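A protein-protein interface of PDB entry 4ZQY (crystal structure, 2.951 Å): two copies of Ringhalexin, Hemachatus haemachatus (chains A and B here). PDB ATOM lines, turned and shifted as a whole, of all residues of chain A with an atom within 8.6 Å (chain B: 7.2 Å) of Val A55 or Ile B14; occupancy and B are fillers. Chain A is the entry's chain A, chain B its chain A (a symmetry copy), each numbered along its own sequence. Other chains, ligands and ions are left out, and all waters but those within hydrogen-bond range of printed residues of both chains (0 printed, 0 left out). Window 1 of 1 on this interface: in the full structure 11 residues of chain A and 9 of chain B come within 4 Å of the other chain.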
ATOM      1  N   CYS A  24      34.573 -11.023 -20.270  1.00  0.00           N
ATOM      2  CA  CYS A  24      34.587 -10.262 -21.508  1.00  0.00           C
ATOM      3  C   CYS A  24      33.317 -10.640 -22.242  1.00  0.00           C
ATOM      4  O   CYS A  24      32.907 -11.795 -22.200  1.00  0.00           O
ATOM      5  CB  CYS A  24      35.791 -10.615 -22.379  1.00  0.00           C
ATOM      6  SG  CYS A  24      37.426 -10.305 -21.727  1.00  0.00           S
ATOM      7  N   PHE A  25      32.663  -9.686 -22.886  1.00  0.00           N
ATOM      8  CA  PHE A  25      31.465 -10.041 -23.631  1.00  0.00           C
ATOM      9  C   PHE A  25      31.592  -9.586 -25.077  1.00  0.00           C
ATOM     10  O   PHE A  25      32.426  -8.741 -25.398  1.00  0.00           O
ATOM     11  CB  PHE A  25      30.208  -9.446 -23.003  1.00  0.00           C
ATOM     12  CG  PHE A  25      30.101  -7.971 -23.161  1.00  0.00           C
ATOM     13  CD1 PHE A  25      29.511  -7.428 -24.291  1.00  0.00           C
ATOM     14  CD2 PHE A  25      30.578  -7.126 -22.187  1.00  0.00           C
ATOM     15  CE1 PHE A  25      29.415  -6.074 -24.447  1.00  0.00           C
ATOM     16  CE2 PHE A  25      30.480  -5.767 -22.339  1.00  0.00           C
ATOM     17  CZ  PHE A  25      29.900  -5.242 -23.470  1.00  0.00           C
ATOM     18  N   LYS A  26      30.731 -10.129 -25.933  1.00  0.00           N
ATOM     19  CA  LYS A  26      30.573  -9.643 -27.297  1.00  0.00           C
ATOM     20  C   LYS A  26      29.102  -9.628 -27.705  1.00  0.00           C
ATOM     21  O   LYS A  26      28.419 -10.641 -27.626  1.00  0.00           O
ATOM     22  CB  LYS A  26      31.368 -10.478 -28.296  1.00  0.00           C
ATOM     23  CG  LYS A  26      31.290  -9.865 -29.685  1.00  0.00           C
ATOM     24  CD  LYS A  26      32.110 -10.575 -30.738  1.00  0.00           C
ATOM     25  CE  LYS A  26      31.403 -11.828 -31.224  1.00  0.00           C
ATOM     26  NZ  LYS A  26      32.054 -12.419 -32.426  1.00  0.00           N
ATOM     27  N   LYS A  27      28.627  -8.475 -28.161  1.00  0.00           N
ATOM     28  CA  LYS A  27      27.231  -8.313 -28.528  1.00  0.00           C
ATOM     29  C   LYS A  27      27.072  -8.090 -30.042  1.00  0.00           C
ATOM     30  O   LYS A  27      27.758  -7.262 -30.631  1.00  0.00           O
ATOM     31  CB  LYS A  27      26.654  -7.122 -27.750  1.00  0.00           C
ATOM     32  CG  LYS A  27      25.167  -7.129 -27.483  1.00  0.00           C
ATOM     33  CD  LYS A  27      24.748  -5.963 -26.567  1.00  0.00           C
ATOM     34  CE  LYS A  27      25.175  -6.212 -25.106  1.00  0.00           C
ATOM     35  NZ  LYS A  27      24.758  -5.138 -24.148  1.00  0.00           N
ATOM     36  N   PHE A  28      26.187  -8.855 -30.677  1.00  0.00           N
ATOM     37  CA  PHE A  28      25.968  -8.712 -32.117  1.00  0.00           C
ATOM     38  C   PHE A  28      24.530  -9.079 -32.500  1.00  0.00           C
ATOM     39  O   PHE A  28      23.890  -9.866 -31.807  1.00  0.00           O
ATOM     40  CB  PHE A  28      26.993  -9.551 -32.895  1.00  0.00           C
ATOM     41  CG  PHE A  28      26.988 -11.011 -32.561  1.00  0.00           C
ATOM     42  CD1 PHE A  28      27.683 -11.493 -31.461  1.00  0.00           C
ATOM     43  CD2 PHE A  28      26.343 -11.911 -33.385  1.00  0.00           C
ATOM     44  CE1 PHE A  28      27.689 -12.838 -31.166  1.00  0.00           C
ATOM     45  CE2 PHE A  28      26.344 -13.262 -33.097  1.00  0.00           C
ATOM     46  CZ  PHE A  28      27.020 -13.729 -31.987  1.00  0.00           C
ATOM     47  N   PRO A  29      24.009  -8.487 -33.591  1.00  0.00           N
ATOM     48  CA  PRO A  29      22.594  -8.685 -33.935  1.00  0.00           C
ATOM     49  C   PRO A  29      22.315 -10.047 -34.556  1.00  0.00           C
ATOM     50  O   PRO A  29      23.259 -10.653 -35.059  1.00  0.00           O
ATOM     51  CB  PRO A  29      22.328  -7.571 -34.947  1.00  0.00           C
ATOM     52  CG  PRO A  29      23.663  -7.334 -35.563  1.00  0.00           C
ATOM     53  CD  PRO A  29      24.654  -7.505 -34.472  1.00  0.00           C
ATOM     54  N   LYS A  30      21.048 -10.469 -34.622  1.00  0.00           N
ATOM     55  CA  LYS A  30      20.771 -11.843 -35.037  1.00  0.00           C
ATOM     56  C   LYS A  30      20.503 -12.092 -36.518  1.00  0.00           C
ATOM     57  O   LYS A  30      20.962 -13.101 -37.057  1.00  0.00           O
ATOM     58  CB  LYS A  30      19.530 -12.361 -34.269  1.00  0.00           C
ATOM     59  CG  LYS A  30      19.773 -13.104 -32.946  1.00  0.00           C
ATOM     60  CD  LYS A  30      18.471 -13.638 -32.260  1.00  0.00           C
ATOM     61  CE  LYS A  30      17.852 -14.907 -32.871  1.00  0.00           C
ATOM     62  NZ  LYS A  30      18.718 -16.123 -32.891  1.00  0.00           N
ATOM     63  N   TRP A  37      26.955  -4.092 -36.808  1.00  0.00           N
ATOM     64  CA  TRP A  37      27.587  -3.563 -35.620  1.00  0.00           C
ATOM     65  C   TRP A  37      27.987  -4.696 -34.679  1.00  0.00           C
ATOM     66  O   TRP A  37      27.309  -5.717 -34.627  1.00  0.00           O
ATOM     67  CB  TRP A  37      26.680  -2.602 -34.868  1.00  0.00           C
ATOM     68  CG  TRP A  37      25.351  -3.157 -34.489  1.00  0.00           C
ATOM     69  CD1 TRP A  37      24.184  -3.045 -35.186  1.00  0.00           C
ATOM     70  CD2 TRP A  37      25.056  -3.959 -33.341  1.00  0.00           C
ATOM     71  NE1 TRP A  37      23.171  -3.687 -34.520  1.00  0.00           N
ATOM     72  CE2 TRP A  37      23.683  -4.266 -33.390  1.00  0.00           C
ATOM     73  CE3 TRP A  37      25.820  -4.437 -32.269  1.00  0.00           C
ATOM     74  CZ2 TRP A  37      23.056  -5.028 -32.411  1.00  0.00           C
ATOM     75  CZ3 TRP A  37      25.197  -5.192 -31.298  1.00  0.00           C
ATOM     76  CH2 TRP A  37      23.828  -5.482 -31.375  1.00  0.00           C
ATOM     77  N   ILE A  39      29.433  -5.165 -30.565  1.00  0.00           N
ATOM     78  CA  ILE A  39      29.815  -4.549 -29.288  1.00  0.00           C
ATOM     79  C   ILE A  39      30.640  -5.456 -28.369  1.00  0.00           C
ATOM     80  O   ILE A  39      30.229  -6.566 -28.060  1.00  0.00           O
ATOM     81  CB  ILE A  39      28.566  -4.110 -28.505  1.00  0.00           C
ATOM     82  CG1 ILE A  39      27.752  -3.134 -29.345  1.00  0.00           C
ATOM     83  CG2 ILE A  39      28.943  -3.443 -27.195  1.00  0.00           C
ATOM     84  CD1 ILE A  39      28.558  -1.943 -29.805  1.00  0.00           C
ATOM     85  N   THR A  45      29.199  -9.458 -14.746  1.00  0.00           N
ATOM     86  CA  THR A  45      28.305 -10.585 -14.995  1.00  0.00           C
ATOM     87  C   THR A  45      27.938 -10.605 -16.476  1.00  0.00           C
ATOM     88  O   THR A  45      27.842  -9.546 -17.103  1.00  0.00           O
ATOM     89  CB  THR A  45      27.011 -10.486 -14.172  1.00  0.00           C
ATOM     90  OG1 THR A  45      26.260  -9.346 -14.605  1.00  0.00           O
ATOM     91  CG2 THR A  45      27.315 -10.358 -12.687  1.00  0.00           C
ATOM     92  N   CYS A  46      27.707 -11.798 -17.022  1.00  0.00           N
ATOM     93  CA  CYS A  46      27.296 -11.938 -18.417  1.00  0.00           C
ATOM     94  C   CYS A  46      26.073 -11.079 -18.689  1.00  0.00           C
ATOM     95  O   CYS A  46      25.037 -11.250 -18.050  1.00  0.00           O
ATOM     96  CB  CYS A  46      26.987 -13.399 -18.763  1.00  0.00           C
ATOM     97  SG  CYS A  46      28.383 -14.539 -18.707  1.00  0.00           S
ATOM     98  N   PRO A  47      26.207 -10.124 -19.624  1.00  0.00           N
ATOM     99  CA  PRO A  47      25.109  -9.239 -20.011  1.00  0.00           C
ATOM    100  C   PRO A  47      23.895 -10.052 -20.424  1.00  0.00           C
ATOM    101  O   PRO A  47      24.068 -11.075 -21.084  1.00  0.00           O
ATOM    102  CB  PRO A  47      25.673  -8.496 -21.227  1.00  0.00           C
ATOM    103  CG  PRO A  47      27.157  -8.589 -21.082  1.00  0.00           C
ATOM    104  CD  PRO A  47      27.413  -9.915 -20.449  1.00  0.00           C
ATOM    105  N   LYS A  48      22.697  -9.630 -20.042  1.00  0.00           N
ATOM    106  CA  LYS A  48      21.499 -10.293 -20.536  1.00  0.00           C
ATOM    107  C   LYS A  48      21.270  -9.856 -21.970  1.00  0.00           C
ATOM    108  O   LYS A  48      21.509  -8.697 -22.301  1.00  0.00           O
ATOM    109  CB  LYS A  48      20.293  -9.924 -19.666  1.00  0.00           C
ATOM    110  CG  LYS A  48      20.488 -10.266 -18.182  1.00  0.00           C
ATOM    111  CD  LYS A  48      21.174 -11.622 -18.004  1.00  0.00           C
ATOM    112  CE  LYS A  48      21.487 -11.909 -16.543  1.00  0.00           C
ATOM    113  NZ  LYS A  48      22.169 -13.224 -16.384  1.00  0.00           N
ATOM    114  N   PRO A  49      20.844 -10.785 -22.839  1.00  0.00           N
ATOM    115  CA  PRO A  49      20.636 -10.413 -24.239  1.00  0.00           C
ATOM    116  C   PRO A  49      19.335  -9.656 -24.451  1.00  0.00           C
ATOM    117  O   PRO A  49      18.427  -9.692 -23.621  1.00  0.00           O
ATOM    118  CB  PRO A  49      20.605 -11.761 -24.956  1.00  0.00           C
ATOM    119  CG  PRO A  49      20.405 -12.793 -23.907  1.00  0.00           C
ATOM    120  CD  PRO A  49      20.400 -12.158 -22.565  1.00  0.00           C
ATOM    121  N   GLU A  50      19.262  -8.999 -25.601  1.00  0.00           N
ATOM    122  CA  GLU A  50      18.109  -8.228 -26.043  1.00  0.00           C
ATOM    123  C   GLU A  50      17.440  -8.960 -27.207  1.00  0.00           C
ATOM    124  O   GLU A  50      18.008  -9.913 -27.737  1.00  0.00           O
ATOM    125  CB  GLU A  50      18.555  -6.822 -26.463  1.00  0.00           C
ATOM    126  CG  GLU A  50      19.111  -5.992 -25.301  1.00  0.00           C
ATOM    127  CD  GLU A  50      20.609  -5.733 -25.427  1.00  0.00           C
ATOM    128  OE1 GLU A  50      21.175  -6.036 -26.497  1.00  0.00           O
ATOM    129  OE2 GLU A  50      21.222  -5.241 -24.455  1.00  0.00           O
ATOM    130  N   ALA A  51      16.241  -8.512 -27.577  1.00  0.00           N
ATOM    131  CA  ALA A  51      15.390  -9.142 -28.603  1.00  0.00           C
ATOM    132  C   ALA A  51      16.146  -9.862 -29.716  1.00  0.00           C
ATOM    133  O   ALA A  51      16.246 -11.094 -29.711  1.00  0.00           O
ATOM    134  CB  ALA A  51      14.453  -8.113 -29.199  1.00  0.00           C
ATOM    135  N   GLN A  52      16.701  -9.090 -30.645  1.00  0.00           N
ATOM    136  CA  GLN A  52      17.376  -9.696 -31.784  1.00  0.00           C
ATOM    137  C   GLN A  52      18.859  -9.548 -31.602  1.00  0.00           C
ATOM    138  O   GLN A  52      19.548  -9.025 -32.474  1.00  0.00           O
ATOM    139  CB  GLN A  52      16.892  -9.079 -33.097  1.00  0.00           C
ATOM    140  CG  GLN A  52      15.511  -9.422 -33.564  1.00  0.00           C
ATOM    141  CD  GLN A  52      15.536 -10.539 -34.578  1.00  0.00           C
ATOM    142  OE1 GLN A  52      16.312 -10.515 -35.531  1.00  0.00           O
ATOM    143  NE2 GLN A  52      14.644 -11.505 -34.407  1.00  0.00           N
ATOM    144  N   VAL A  53      19.361 -10.045 -30.479  1.00  0.00           N
ATOM    145  CA  VAL A  53      20.772  -9.927 -30.172  1.00  0.00           C
ATOM    146  C   VAL A  53      21.305 -11.182 -29.485  1.00  0.00           C
ATOM    147  O   VAL A  53      20.630 -11.752 -28.628  1.00  0.00           O
ATOM    148  CB  VAL A  53      21.014  -8.707 -29.227  1.00  0.00           C
ATOM    149  CG1 VAL A  53      22.396  -8.761 -28.627  1.00  0.00           C
ATOM    150  CG2 VAL A  53      20.786  -7.374 -29.944  1.00  0.00           C
ATOM    151  N   TYR A  54      22.501 -11.618 -29.880  1.00  0.00           N
ATOM    152  CA  TYR A  54      23.274 -12.609 -29.128  1.00  0.00           C
ATOM    153  C   TYR A  54      24.312 -11.905 -28.243  1.00  0.00           C
ATOM    154  O   TYR A  54      24.797 -10.832 -28.609  1.00  0.00           O
ATOM    155  CB  TYR A  54      24.022 -13.572 -30.055  1.00  0.00           C
ATOM    156  CG  TYR A  54      23.182 -14.452 -30.955  1.00  0.00           C
ATOM    157  CD1 TYR A  54      22.512 -15.552 -30.448  1.00  0.00           C
ATOM    158  CD2 TYR A  54      23.147 -14.245 -32.333  1.00  0.00           C
ATOM    159  CE1 TYR A  54      21.765 -16.373 -31.268  1.00  0.00           C
ATOM    160  CE2 TYR A  54      22.418 -15.074 -33.158  1.00  0.00           C
ATOM    161  CZ  TYR A  54      21.727 -16.138 -32.618  1.00  0.00           C
ATOM    162  OH  TYR A  54      20.979 -16.976 -33.414  1.00  0.00           O
ATOM    163  N   VAL A  55      24.641 -12.481 -27.082  1.00  0.00           N
ATOM    164  CA  VAL A  55      25.782 -11.983 -26.296  1.00  0.00           C
ATOM    165  C   VAL A  55      26.691 -13.179 -26.023  1.00  0.00           C
ATOM    166  O   VAL A  55      26.266 -14.222 -25.541  1.00  0.00           O
ATOM    167  CB  VAL A  55      25.392 -11.230 -24.971  1.00  0.00           C
ATOM    168  CG1 VAL A  55      24.122 -10.425 -25.165  1.00  0.00           C
ATOM    169  CG2 VAL A  55      25.247 -12.161 -23.796  1.00  0.00           C
ATOM    170  N   ASP A  56      27.940 -13.053 -26.429  1.00  0.00           N
ATOM    171  CA  ASP A  56      28.933 -14.034 -26.063  1.00  0.00           C
ATOM    172  C   ASP A  56      29.438 -13.570 -24.722  1.00  0.00           C
ATOM    173  O   ASP A  56      29.547 -12.374 -24.473  1.00  0.00           O
ATOM    174  CB  ASP A  56      30.098 -14.098 -27.050  1.00  0.00           C
ATOM    175  CG  ASP A  56      29.665 -14.531 -28.432  1.00  0.00           C
ATOM    176  OD1 ASP A  56      28.492 -14.923 -28.581  1.00  0.00           O
ATOM    177  OD2 ASP A  56      30.497 -14.494 -29.365  1.00  0.00           O
ATOM    178  N   CYS A  57      29.684 -14.517 -23.833  1.00  0.00           N
ATOM    179  CA  CYS A  57      30.259 -14.190 -22.550  1.00  0.00           C
ATOM    180  C   CYS A  57      31.346 -15.216 -22.255  1.00  0.00           C
ATOM    181  O   CYS A  57      31.093 -16.416 -22.304  1.00  0.00           O
ATOM    182  CB  CYS A  57      29.168 -14.184 -21.471  1.00  0.00           C
ATOM    183  SG  CYS A  57      29.645 -13.498 -19.897  1.00  0.00           S
ATOM    184  N   CYS A  58      32.567 -14.743 -22.024  1.00  0.00           N
ATOM    185  CA  CYS A  58      33.702 -15.627 -21.764  1.00  0.00           C
ATOM    186  C   CYS A  58      34.576 -15.020 -20.665  1.00  0.00           C
ATOM    187  O   CYS A  58      34.384 -13.866 -20.289  1.00  0.00           O
ATOM    188  CB  CYS A  58      34.507 -15.865 -23.053  1.00  0.00           C
ATOM    189  SG  CYS A  58      35.197 -14.410 -23.888  1.00  0.00           S
ATOM    190  N   ASN A  64      36.880 -12.522 -26.185  1.00  0.00           N
ATOM    191  CA  ASN A  64      35.706 -12.166 -26.983  1.00  0.00           C
ATOM    192  C   ASN A  64      36.001 -11.769 -28.433  1.00  0.00           C
ATOM    193  O   ASN A  64      35.839 -10.612 -28.797  1.00  0.00           O
ATOM    194  CB  ASN A  64      34.880 -11.075 -26.264  1.00  0.00           C
ATOM    195  CG  ASN A  64      35.703  -9.850 -25.868  1.00  0.00           C
ATOM    196  OD1 ASN A  64      36.890  -9.955 -25.541  1.00  0.00           O
ATOM    197  ND2 ASN A  64      35.053  -8.688 -25.838  1.00  0.00           N
ATOM    198  N   LEU B   2      15.735 -17.928 -21.526  1.00  0.00           N
ATOM    199  CA  LEU B   2      17.059 -17.773 -22.094  1.00  0.00           C
ATOM    200  C   LEU B   2      17.656 -19.110 -22.441  1.00  0.00           C
ATOM    201  O   LEU B   2      17.627 -20.044 -21.640  1.00  0.00           O
ATOM    202  CB  LEU B   2      17.997 -17.070 -21.117  1.00  0.00           C
ATOM    203  CG  LEU B   2      17.776 -15.636 -20.668  1.00  0.00           C
ATOM    204  CD1 LEU B   2      18.972 -15.229 -19.861  1.00  0.00           C
ATOM    205  CD2 LEU B   2      17.577 -14.713 -21.847  1.00  0.00           C
ATOM    206  N   CYS B   3      18.136 -19.205 -23.671  1.00  0.00           N
ATOM    207  CA  CYS B   3      18.745 -20.415 -24.188  1.00  0.00           C
ATOM    208  C   CYS B   3      20.148 -20.109 -24.647  1.00  0.00           C
ATOM    209  O   CYS B   3      20.523 -18.949 -24.797  1.00  0.00           O
ATOM    210  CB  CYS B   3      17.935 -20.990 -25.337  1.00  0.00           C
ATOM    211  SG  CYS B   3      16.294 -21.471 -24.853  1.00  0.00           S
ATOM    212  N   LEU B   4      20.917 -21.168 -24.858  1.00  0.00           N
ATOM    213  CA  LEU B   4      22.263 -21.048 -25.367  1.00  0.00           C
ATOM    214  C   LEU B   4      22.212 -21.153 -26.873  1.00  0.00           C
ATOM    215  O   LEU B   4      21.391 -21.889 -27.422  1.00  0.00           O
ATOM    216  CB  LEU B   4      23.157 -22.128 -24.782  1.00  0.00           C
ATOM    217  CG  LEU B   4      23.387 -22.048 -23.280  1.00  0.00           C
ATOM    218  CD1 LEU B   4      24.225 -23.232 -22.844  1.00  0.00           C
ATOM    219  CD2 LEU B   4      24.088 -20.743 -22.957  1.00  0.00           C
ATOM    220  N   SER B   5      23.085 -20.411 -27.542  1.00  0.00           N
ATOM    221  CA  SER B   5      23.178 -20.498 -28.989  1.00  0.00           C
ATOM    222  C   SER B   5      24.411 -21.317 -29.320  1.00  0.00           C
ATOM    223  O   SER B   5      24.448 -22.041 -30.318  1.00  0.00           O
ATOM    224  CB  SER B   5      23.280 -19.109 -29.592  1.00  0.00           C
ATOM    225  OG  SER B   5      22.150 -18.358 -29.193  1.00  0.00           O
ATOM    226  N   ASP B   6      25.428 -21.165 -28.472  1.00  0.00           N
ATOM    227  CA  ASP B   6      26.664 -21.915 -28.589  1.00  0.00           C
ATOM    228  C   ASP B   6      27.172 -22.129 -27.168  1.00  0.00           C
ATOM    229  O   ASP B   6      26.878 -21.330 -26.274  1.00  0.00           O
ATOM    230  CB  ASP B   6      27.690 -21.197 -29.462  1.00  0.00           C
ATOM    231  CG  ASP B   6      28.818 -22.121 -29.886  1.00  0.00           C
ATOM    232  OD1 ASP B   6      28.597 -22.920 -30.820  1.00  0.00           O
ATOM    233  OD2 ASP B   6      29.912 -22.068 -29.278  1.00  0.00           O
ATOM    234  N   PHE B  10      34.667 -22.151 -21.394  1.00  0.00           N
ATOM    235  CA  PHE B  10      33.517 -21.369 -20.975  1.00  0.00           C
ATOM    236  C   PHE B  10      33.432 -20.181 -21.922  1.00  0.00           C
ATOM    237  O   PHE B  10      33.916 -19.087 -21.638  1.00  0.00           O
ATOM    238  CB  PHE B  10      33.554 -20.936 -19.506  1.00  0.00           C
ATOM    239  CG  PHE B  10      32.362 -20.099 -19.081  1.00  0.00           C
ATOM    240  CD1 PHE B  10      31.124 -20.692 -18.873  1.00  0.00           C
ATOM    241  CD2 PHE B  10      32.485 -18.732 -18.873  1.00  0.00           C
ATOM    242  CE1 PHE B  10      30.035 -19.936 -18.475  1.00  0.00           C
ATOM    243  CE2 PHE B  10      31.396 -17.969 -18.478  1.00  0.00           C
ATOM    244  CZ  PHE B  10      30.174 -18.569 -18.278  1.00  0.00           C
ATOM    245  N   GLU B  12      29.977 -19.129 -23.744  1.00  0.00           N
ATOM    246  CA  GLU B  12      28.584 -19.375 -24.062  1.00  0.00           C
ATOM    247  C   GLU B  12      27.928 -18.207 -24.786  1.00  0.00           C
ATOM    248  O   GLU B  12      28.139 -17.052 -24.435  1.00  0.00           O
ATOM    249  CB  GLU B  12      27.804 -19.704 -22.791  1.00  0.00           C
ATOM    250  CG  GLU B  12      27.982 -18.706 -21.681  1.00  0.00           C
ATOM    251  CD  GLU B  12      27.205 -19.089 -20.441  1.00  0.00           C
ATOM    252  OE1 GLU B  12      27.343 -20.247 -19.977  1.00  0.00           O
ATOM    253  OE2 GLU B  12      26.470 -18.216 -19.926  1.00  0.00           O
ATOM    254  N   THR B  13      27.193 -18.519 -25.846  1.00  0.00           N
ATOM    255  CA  THR B  13      26.428 -17.513 -26.566  1.00  0.00           C
ATOM    256  C   THR B  13      24.971 -17.589 -26.122  1.00  0.00           C
ATOM    257  O   THR B  13      24.313 -18.614 -26.286  1.00  0.00           O
ATOM    258  CB  THR B  13      26.519 -17.721 -28.086  1.00  0.00           C
ATOM    259  OG1 THR B  13      27.895 -17.718 -28.494  1.00  0.00           O
ATOM    260  CG2 THR B  13      25.765 -16.619 -28.815  1.00  0.00           C
ATOM    261  N   ILE B  14      24.464 -16.489 -25.580  1.00  0.00           N
ATOM    262  CA  ILE B  14      23.147 -16.486 -24.964  1.00  0.00           C
ATOM    263  C   ILE B  14      22.156 -15.675 -25.792  1.00  0.00           C
ATOM    264  O   ILE B  14      22.463 -14.574 -26.253  1.00  0.00           O
ATOM    265  CB  ILE B  14      23.206 -15.901 -23.547  1.00  0.00           C
ATOM    266  CG1 ILE B  14      24.377 -16.504 -22.768  1.00  0.00           C
ATOM    267  CG2 ILE B  14      21.876 -16.075 -22.833  1.00  0.00           C
ATOM    268  CD1 ILE B  14      25.443 -15.485 -22.366  1.00  0.00           C
ATOM    269  N   GLU B  15      20.947 -16.201 -25.926  1.00  0.00           N
ATOM    270  CA  GLU B  15      19.851 -15.481 -26.548  1.00  0.00           C
ATOM    271  C   GLU B  15      18.605 -15.467 -25.677  1.00  0.00           C
ATOM    272  O   GLU B  15      18.473 -16.264 -24.743  1.00  0.00           O
ATOM    273  CB  GLU B  15      19.522 -16.093 -27.905  1.00  0.00           C
ATOM    274  CG  GLU B  15      19.044 -17.533 -27.850  1.00  0.00           C
ATOM    275  CD  GLU B  15      18.591 -18.025 -29.208  1.00  0.00           C
ATOM    276  OE1 GLU B  15      17.654 -17.430 -29.775  1.00  0.00           O
ATOM    277  OE2 GLU B  15      19.201 -18.977 -29.730  1.00  0.00           O
ATOM    278  N   ILE B  16      17.738 -14.494 -25.933  1.00  0.00           N
ATOM    279  CA  ILE B  16      16.451 -14.413 -25.252  1.00  0.00           C
ATOM    280  C   ILE B  16      15.325 -14.941 -26.166  1.00  0.00           C
ATOM    281  O   ILE B  16      15.208 -14.559 -27.329  1.00  0.00           O
ATOM    282  CB  ILE B  16      16.176 -12.973 -24.751  1.00  0.00           C
ATOM    283  CG1 ILE B  16      14.850 -12.903 -23.995  1.00  0.00           C
ATOM    284  CG2 ILE B  16      16.322 -11.936 -25.863  1.00  0.00           C
ATOM    285  CD1 ILE B  16      14.693 -11.635 -23.221  1.00  0.00           C
ATOM    286  N   LYS B  62      19.271 -21.295 -20.069  1.00  0.00           N
ATOM    287  CA  LYS B  62      20.629 -21.668 -20.473  1.00  0.00           C
ATOM    288  C   LYS B  62      20.907 -23.118 -20.129  1.00  0.00           C
ATOM    289  O   LYS B  62      22.025 -23.476 -19.745  1.00  0.00           O
ATOM    290  CB  LYS B  62      21.663 -20.713 -19.844  1.00  0.00           C
ATOM    291  CG  LYS B  62      21.516 -19.297 -20.363  1.00  0.00           C
ATOM    292  CD  LYS B  62      22.418 -18.245 -19.737  1.00  0.00           C
ATOM    293  CE  LYS B  62      23.307 -18.718 -18.616  1.00  0.00           C
ATOM    294  NZ  LYS B  62      24.126 -17.546 -18.153  1.00  0.00           N
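OE1 of Glu B15 lies within salt-bridge range of NZ of Lys A30. The backbone carbonyl oxygen (O) of Val A55 is in hydrogen-bond range of the backbone NH (N) of Ile B14. OG1 of Thr B13 sits at hydrogen-bond distance from OD1 of Asp A56, 2.9 Å away. The backbone carbonyl oxygen (O) of Glu B12 lies within hydrogen-bond range of the backbone NH (N) of Cys A57.
The side-chain amino group (NZ) of Lys A27 is in salt-bridge range of the side-chain carboxylate (OE2) of Glu A50 (3.6 Å). N of Lys A30 lies within hydrogen-bond range of O of Gln A52 (3.0 Å). The side-chain sulfur (SG) of Cys A57 forms a disulfide with the side-chain sulfur (SG) of Cys A46. The backbone NH of Glu B15 sits at hydrogen-bond distance from the backbone carbonyl oxygen of Cys B3. N of Thr B13 is in hydrogen-bond range of O of Asp B6 (2.9 Å). NZ of Lys B62 lies within salt-bridge range of OE2 of Glu B12 (3.0 Å).
Pro A49 touches Leu B2. CG of Pro A49 touches N of Ile B16, at 3.8 Å. CG2 of Ile B16 touches O of Glu A50, 3.2 Å away. Ala A51 touches Ile B16. Ser B5 touches Tyr A54. Tyr A54 touches Thr B13. Glu B15 touches Tyr A54 (CB to CD1, 3.96 Å). Val A55 touches Thr B13. Asp A56 touches Glu B12. CA of Cys A58 touches O of Phe B10 (3.5 Å).
Phe A28 touches none of the printed residues of chain B. Printed residues of chain B within 4 Å of Glu A50: Ile B16 (3.2 Å). Printed residues of chain B within 4 Å of Ala A51: Ile B16 (3.8 Å). Val A55 touches just these residues of chain B: Glu B12, Thr B13 and Ile B14. Printed residues of chain B within 4 Å of Asp A56: Glu B12 and Thr B13. Printed residues of chain A within 4 Å of Thr B13: Tyr A54 (3.7 Å), Val A55 (3.5 Å) and Asp A56 (2.9 Å). Of the printed residues of chain A, Ile B14 touches Pro A49, Tyr A54 and Val A55. The nearest residue of chain A that does not touch Ile B14 is Cys A57 (4.05 Å). The nearest printed residue of chain A that does not touch Ser B5 is Lys A30 (5.5 Å).
Of the 12 printed residues of chain B, 8 touch a printed residue of chain A. Printed residues of chain A that touch a printed residue of chain B: Lys A30, Pro A49, Glu A50, Ala A51, Tyr A54, Val A55, Asp A56, Cys A57 and Cys A58. Hydrophobic or aromatic side chains of chain A within 4 Å of the printed part of chain B: Pro A49, Tyr A54 and Val A55. Along chain A the printed residues that touch a printed residue of chain B span positions 30 to 58. Among the printed residues, Asp or Glu carboxylates within 4 Å of a Lys or Arg side-chain nitrogen of the other chain: Lys A30 with Glu B15.
No position is printed for both chains.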
